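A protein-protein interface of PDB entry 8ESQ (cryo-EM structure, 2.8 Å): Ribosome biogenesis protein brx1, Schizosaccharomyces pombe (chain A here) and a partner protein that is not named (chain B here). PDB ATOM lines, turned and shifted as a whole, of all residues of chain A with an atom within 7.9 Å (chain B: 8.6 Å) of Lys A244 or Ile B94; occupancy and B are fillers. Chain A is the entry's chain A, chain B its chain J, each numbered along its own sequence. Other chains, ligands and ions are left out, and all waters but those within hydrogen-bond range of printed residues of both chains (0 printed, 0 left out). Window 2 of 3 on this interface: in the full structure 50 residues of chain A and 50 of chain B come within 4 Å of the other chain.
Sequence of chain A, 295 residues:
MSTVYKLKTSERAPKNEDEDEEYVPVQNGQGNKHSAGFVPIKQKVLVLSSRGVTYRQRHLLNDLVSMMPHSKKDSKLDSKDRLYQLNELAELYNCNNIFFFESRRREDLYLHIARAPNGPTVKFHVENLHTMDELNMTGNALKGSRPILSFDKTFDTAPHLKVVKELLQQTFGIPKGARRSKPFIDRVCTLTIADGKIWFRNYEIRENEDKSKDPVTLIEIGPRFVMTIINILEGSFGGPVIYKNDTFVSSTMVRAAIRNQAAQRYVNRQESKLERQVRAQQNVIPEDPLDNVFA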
ATOM      1  N   HIS A 160      19.994   8.888  11.320  1.00  0.00           N
ATOM      2  CA  HIS A 160      20.873   9.893  11.911  1.00  0.00           C
ATOM      3  C   HIS A 160      21.821  10.466  10.869  1.00  0.00           C
ATOM      4  O   HIS A 160      22.113  11.668  10.877  1.00  0.00           O
ATOM      5  CB  HIS A 160      21.649   9.298  13.089  1.00  0.00           C
ATOM      6  CG  HIS A 160      22.817   8.451  12.691  1.00  0.00           C
ATOM      7  ND1 HIS A 160      22.705   7.102  12.433  1.00  0.00           N
ATOM      8  CD2 HIS A 160      24.126   8.758  12.529  1.00  0.00           C
ATOM      9  CE1 HIS A 160      23.893   6.617  12.117  1.00  0.00           C
ATOM     10  NE2 HIS A 160      24.772   7.602  12.170  1.00  0.00           N
ATOM     11  N   ILE A 229      30.811  12.010  14.373  1.00  0.00           N
ATOM     12  CA  ILE A 229      29.611  12.211  15.178  1.00  0.00           C
ATOM     13  C   ILE A 229      29.778  11.507  16.514  1.00  0.00           C
ATOM     14  O   ILE A 229      30.254  10.367  16.577  1.00  0.00           O
ATOM     15  CB  ILE A 229      28.374  11.696  14.427  1.00  0.00           C
ATOM     16  CG1 ILE A 229      28.200  12.444  13.106  1.00  0.00           C
ATOM     17  CG2 ILE A 229      27.128  11.846  15.277  1.00  0.00           C
ATOM     18  CD1 ILE A 229      27.207  11.797  12.171  1.00  0.00           C
ATOM     19  N   ILE A 230      29.398  12.184  17.597  1.00  0.00           N
ATOM     20  CA  ILE A 230      29.497  11.635  18.943  1.00  0.00           C
ATOM     21  C   ILE A 230      28.121  11.432  19.570  1.00  0.00           C
ATOM     22  O   ILE A 230      27.821  10.355  20.085  1.00  0.00           O
ATOM     23  CB  ILE A 230      30.397  12.513  19.839  1.00  0.00           C
ATOM     24  CG1 ILE A 230      31.865  12.244  19.509  1.00  0.00           C
ATOM     25  CG2 ILE A 230      30.117  12.241  21.308  1.00  0.00           C
ATOM     26  CD1 ILE A 230      32.832  12.818  20.506  1.00  0.00           C
ATOM     27  N   ASN A 231      27.274  12.456  19.540  1.00  0.00           N
ATOM     28  CA  ASN A 231      25.911  12.294  20.029  1.00  0.00           C
ATOM     29  C   ASN A 231      25.007  13.299  19.332  1.00  0.00           C
ATOM     30  O   ASN A 231      25.471  14.268  18.727  1.00  0.00           O
ATOM     31  CB  ASN A 231      25.827  12.438  21.557  1.00  0.00           C
ATOM     32  CG  ASN A 231      26.172  13.836  22.049  1.00  0.00           C
ATOM     33  OD1 ASN A 231      26.571  14.702  21.278  1.00  0.00           O
ATOM     34  ND2 ASN A 231      26.006  14.059  23.347  1.00  0.00           N
ATOM     35  N   ILE A 232      23.704  13.041  19.415  1.00  0.00           N
ATOM     36  CA  ILE A 232      22.689  13.903  18.824  1.00  0.00           C
ATOM     37  C   ILE A 232      21.603  14.134  19.864  1.00  0.00           C
ATOM     38  O   ILE A 232      21.117  13.182  20.480  1.00  0.00           O
ATOM     39  CB  ILE A 232      22.085  13.293  17.544  1.00  0.00           C
ATOM     40  CG1 ILE A 232      23.158  13.122  16.471  1.00  0.00           C
ATOM     41  CG2 ILE A 232      20.967  14.171  17.013  1.00  0.00           C
ATOM     42  CD1 ILE A 232      22.627  12.586  15.163  1.00  0.00           C
ATOM     43  N   PRO A 240      16.922  15.184  25.677  1.00  0.00           N
ATOM     44  CA  PRO A 240      17.383  13.792  25.741  1.00  0.00           C
ATOM     45  C   PRO A 240      18.133  13.384  24.481  1.00  0.00           C
ATOM     46  O   PRO A 240      17.811  13.817  23.373  1.00  0.00           O
ATOM     47  CB  PRO A 240      16.083  12.995  25.904  1.00  0.00           C
ATOM     48  CG  PRO A 240      15.019  13.890  25.371  1.00  0.00           C
ATOM     49  CD  PRO A 240      15.454  15.282  25.713  1.00  0.00           C
ATOM     50  N   VAL A 241      19.145  12.537  24.668  1.00  0.00           N
ATOM     51  CA  VAL A 241      19.928  12.037  23.547  1.00  0.00           C
ATOM     52  C   VAL A 241      19.063  11.125  22.688  1.00  0.00           C
ATOM     53  O   VAL A 241      18.307  10.288  23.200  1.00  0.00           O
ATOM     54  CB  VAL A 241      21.179  11.300  24.054  1.00  0.00           C
ATOM     55  CG1 VAL A 241      22.102  10.959  22.898  1.00  0.00           C
ATOM     56  CG2 VAL A 241      21.904  12.137  25.094  1.00  0.00           C
ATOM     57  N   ILE A 242      19.162  11.288  21.371  1.00  0.00           N
ATOM     58  CA  ILE A 242      18.428  10.448  20.437  1.00  0.00           C
ATOM     59  C   ILE A 242      19.337   9.529  19.629  1.00  0.00           C
ATOM     60  O   ILE A 242      18.843   8.537  19.071  1.00  0.00           O
ATOM     61  CB  ILE A 242      17.548  11.293  19.494  1.00  0.00           C
ATOM     62  CG1 ILE A 242      18.371  12.403  18.840  1.00  0.00           C
ATOM     63  CG2 ILE A 242      16.364  11.872  20.252  1.00  0.00           C
ATOM     64  CD1 ILE A 242      17.596  13.228  17.839  1.00  0.00           C
ATOM     65  N   TYR A 243      20.633   9.823  19.539  1.00  0.00           N
ATOM     66  CA  TYR A 243      21.593   8.908  18.940  1.00  0.00           C
ATOM     67  C   TYR A 243      22.893   8.964  19.725  1.00  0.00           C
ATOM     68  O   TYR A 243      23.378  10.048  20.059  1.00  0.00           O
ATOM     69  CB  TYR A 243      21.867   9.236  17.467  1.00  0.00           C
ATOM     70  CG  TYR A 243      23.178   8.668  16.965  1.00  0.00           C
ATOM     71  CD1 TYR A 243      23.284   7.332  16.612  1.00  0.00           C
ATOM     72  CD2 TYR A 243      24.307   9.468  16.845  1.00  0.00           C
ATOM     73  CE1 TYR A 243      24.477   6.805  16.156  1.00  0.00           C
ATOM     74  CE2 TYR A 243      25.504   8.949  16.390  1.00  0.00           C
ATOM     75  CZ  TYR A 243      25.583   7.618  16.046  1.00  0.00           C
ATOM     76  OH  TYR A 243      26.774   7.099  15.591  1.00  0.00           O
ATOM     77  N   LYS A 244      23.457   7.793  20.007  1.00  0.00           N
ATOM     78  CA  LYS A 244      24.747   7.677  20.674  1.00  0.00           C
ATOM     79  C   LYS A 244      25.684   6.869  19.790  1.00  0.00           C
ATOM     80  O   LYS A 244      25.286   5.841  19.233  1.00  0.00           O
ATOM     81  CB  LYS A 244      24.604   7.019  22.048  1.00  0.00           C
ATOM     82  CG  LYS A 244      25.917   6.843  22.790  1.00  0.00           C
ATOM     83  CD  LYS A 244      26.509   8.186  23.186  1.00  0.00           C
ATOM     84  CE  LYS A 244      28.024   8.121  23.257  1.00  0.00           C
ATOM     85  NZ  LYS A 244      28.499   7.437  24.490  1.00  0.00           N
ATOM     86  N   ASN A 245      26.922   7.337  19.662  1.00  0.00           N
ATOM     87  CA  ASN A 245      27.906   6.679  18.810  1.00  0.00           C
ATOM     88  C   ASN A 245      28.253   5.288  19.332  1.00  0.00           C
ATOM     89  O   ASN A 245      28.740   5.138  20.452  1.00  0.00           O
ATOM     90  CB  ASN A 245      29.171   7.531  18.702  1.00  0.00           C
ATOM     91  CG  ASN A 245      29.993   7.199  17.474  1.00  0.00           C
ATOM     92  OD1 ASN A 245      29.568   6.422  16.622  1.00  0.00           O
ATOM     93  ND2 ASN A 245      31.179   7.786  17.380  1.00  0.00           N
ATOM     94  N   ILE B  94      18.274   6.233  21.657  1.00  0.00           N
ATOM     95  CA  ILE B  94      19.463   5.562  21.147  1.00  0.00           C
ATOM     96  C   ILE B  94      19.175   4.978  19.769  1.00  0.00           C
ATOM     97  O   ILE B  94      18.570   3.911  19.657  1.00  0.00           O
ATOM     98  CB  ILE B  94      19.946   4.471  22.117  1.00  0.00           C
ATOM     99  CG1 ILE B  94      20.213   5.068  23.501  1.00  0.00           C
ATOM    100  CG2 ILE B  94      21.194   3.790  21.577  1.00  0.00           C
ATOM    101  CD1 ILE B  94      21.485   5.878  23.588  1.00  0.00           C
ATOM    102  N   ASN B  95      19.611   5.691  18.729  1.00  0.00           N
ATOM    103  CA  ASN B  95      19.406   5.272  17.341  1.00  0.00           C
ATOM    104  C   ASN B  95      17.926   5.030  17.051  1.00  0.00           C
ATOM    105  O   ASN B  95      17.553   4.103  16.328  1.00  0.00           O
ATOM    106  CB  ASN B  95      20.245   4.032  17.015  1.00  0.00           C
ATOM    107  CG  ASN B  95      21.677   4.375  16.631  1.00  0.00           C
ATOM    108  OD1 ASN B  95      21.951   4.767  15.496  1.00  0.00           O
ATOM    109  ND2 ASN B  95      22.596   4.232  17.580  1.00  0.00           N
ATOM    110  N   ASN B  96      17.073   5.884  17.614  1.00  0.00           N
ATOM    111  CA  ASN B  96      15.624   5.754  17.464  1.00  0.00           C
ATOM    112  C   ASN B  96      15.294   6.182  16.040  1.00  0.00           C
ATOM    113  O   ASN B  96      15.239   7.374  15.732  1.00  0.00           O
ATOM    114  CB  ASN B  96      14.915   6.595  18.528  1.00  0.00           C
ATOM    115  CG  ASN B  96      13.446   6.946  18.195  1.00  0.00           C
ATOM    116  OD1 ASN B  96      12.959   6.792  17.077  1.00  0.00           O
ATOM    117  ND2 ASN B  96      12.740   7.434  19.209  1.00  0.00           N
ATOM    118  N   THR B  97      15.086   5.199  15.162  1.00  0.00           N
ATOM    119  CA  THR B  97      14.890   5.493  13.746  1.00  0.00           C
ATOM    120  C   THR B  97      13.610   6.286  13.502  1.00  0.00           C
ATOM    121  O   THR B  97      13.614   7.256  12.734  1.00  0.00           O
ATOM    122  CB  THR B  97      14.876   4.191  12.943  1.00  0.00           C
ATOM    123  OG1 THR B  97      16.132   3.519  13.100  1.00  0.00           O
ATOM    124  CG2 THR B  97      14.629   4.465  11.467  1.00  0.00           C
ATOM    125  N   VAL B  98      12.508   5.896  14.147  1.00  0.00           N
ATOM    126  CA  VAL B  98      11.205   6.457  13.789  1.00  0.00           C
ATOM    127  C   VAL B  98      11.147   7.949  14.105  1.00  0.00           C
ATOM    128  O   VAL B  98      10.709   8.754  13.276  1.00  0.00           O
ATOM    129  CB  VAL B  98      10.067   5.670  14.469  1.00  0.00           C
ATOM    130  CG1 VAL B  98      10.184   5.700  15.989  1.00  0.00           C
ATOM    131  CG2 VAL B  98       8.716   6.214  14.025  1.00  0.00           C
ATOM    132  N   LEU B 100      13.840   9.814  14.510  1.00  0.00           N
ATOM    133  CA  LEU B 100      14.883  10.396  13.672  1.00  0.00           C
ATOM    134  C   LEU B 100      14.388  10.595  12.247  1.00  0.00           C
ATOM    135  O   LEU B 100      14.758  11.570  11.581  1.00  0.00           O
ATOM    136  CB  LEU B 100      16.119   9.501  13.701  1.00  0.00           C
ATOM    137  CG  LEU B 100      17.313  10.049  14.472  1.00  0.00           C
ATOM    138  CD1 LEU B 100      16.927  10.282  15.916  1.00  0.00           C
ATOM    139  CD2 LEU B 100      18.427   9.041  14.406  1.00  0.00           C
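O of Ile A242 lies within hydrogen-bond range of N of Asn B95 (3.0 Å).
N of Ile A232 sits at hydrogen-bond distance from O of Tyr A243 (3.1 Å).
The side-chain amide oxygen (OD1) of Asn B96 is in hydrogen-bond range of the backbone NH (N) of Val B98, at 3.1 Å.
N of Ile A242 sits at hydrogen-bond distance from O of Ile A232 (2.9 Å).
The side-chain hydroxyl (OH) of Tyr A243 lies within hydrogen-bond range of the side-chain amide oxygen (OD1) of Asn A245.
Among the printed residues, pairs that only touch across the chains: Tyr A243 with Asn B95, His A160 with Leu B100, Ile A242 with Asn B96, Ile A242 with Ile B94, Lys A244 with Asn B95, Ile A242 with Leu B100, Lys A244 with Ile B94 and His A160 with Asn B95.
Printed residues of chain B within 4 Å of Ile A242: Ile B94 (3.5 Å), Asn B95 (3.0 Å), Asn B96 (3.5 Å) and Leu B100 (3.6 Å).
Printed residues of chain B within 4 Å of Tyr A243: Asn B95 (3.1 Å).
Lys A244 touches just these residues of chain B: Ile B94 and Asn B95.
Of chain A, only Ile A242 (3.5 Å) and Lys A244 (3.7 Å) come within 4 Å of Ile B94.
Of the printed residues of chain A, Asn B96 touches Ile A242.
Printed residues of chain A within 4 Å of Leu B100: His A160 (3.5 Å) and Ile A242 (3.6 Å).
The nearest residue of chain B that does not touch Lys A244 is Asn B96 (7.1 Å).
The nearest residue of chain A that does not touch Ile B94 is Val A241 (4.3 Å).
The nearest printed residue of chain B that does not touch His A160 is Thr B97 (6.6 Å).
Along chain A the printed residues that touch a printed residue of chain B span positions 160 to 244.
Of the 6 printed residues of chain B, 4 touch a printed residue of chain A.
Printed residues of chain B that touch a printed residue of chain A: Ile B94, Asn B95, Asn B96 and Leu B100.
Hydrophobic or aromatic side chains of chain B that line the printed part of chain A: Ile B94 and Leu B100.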
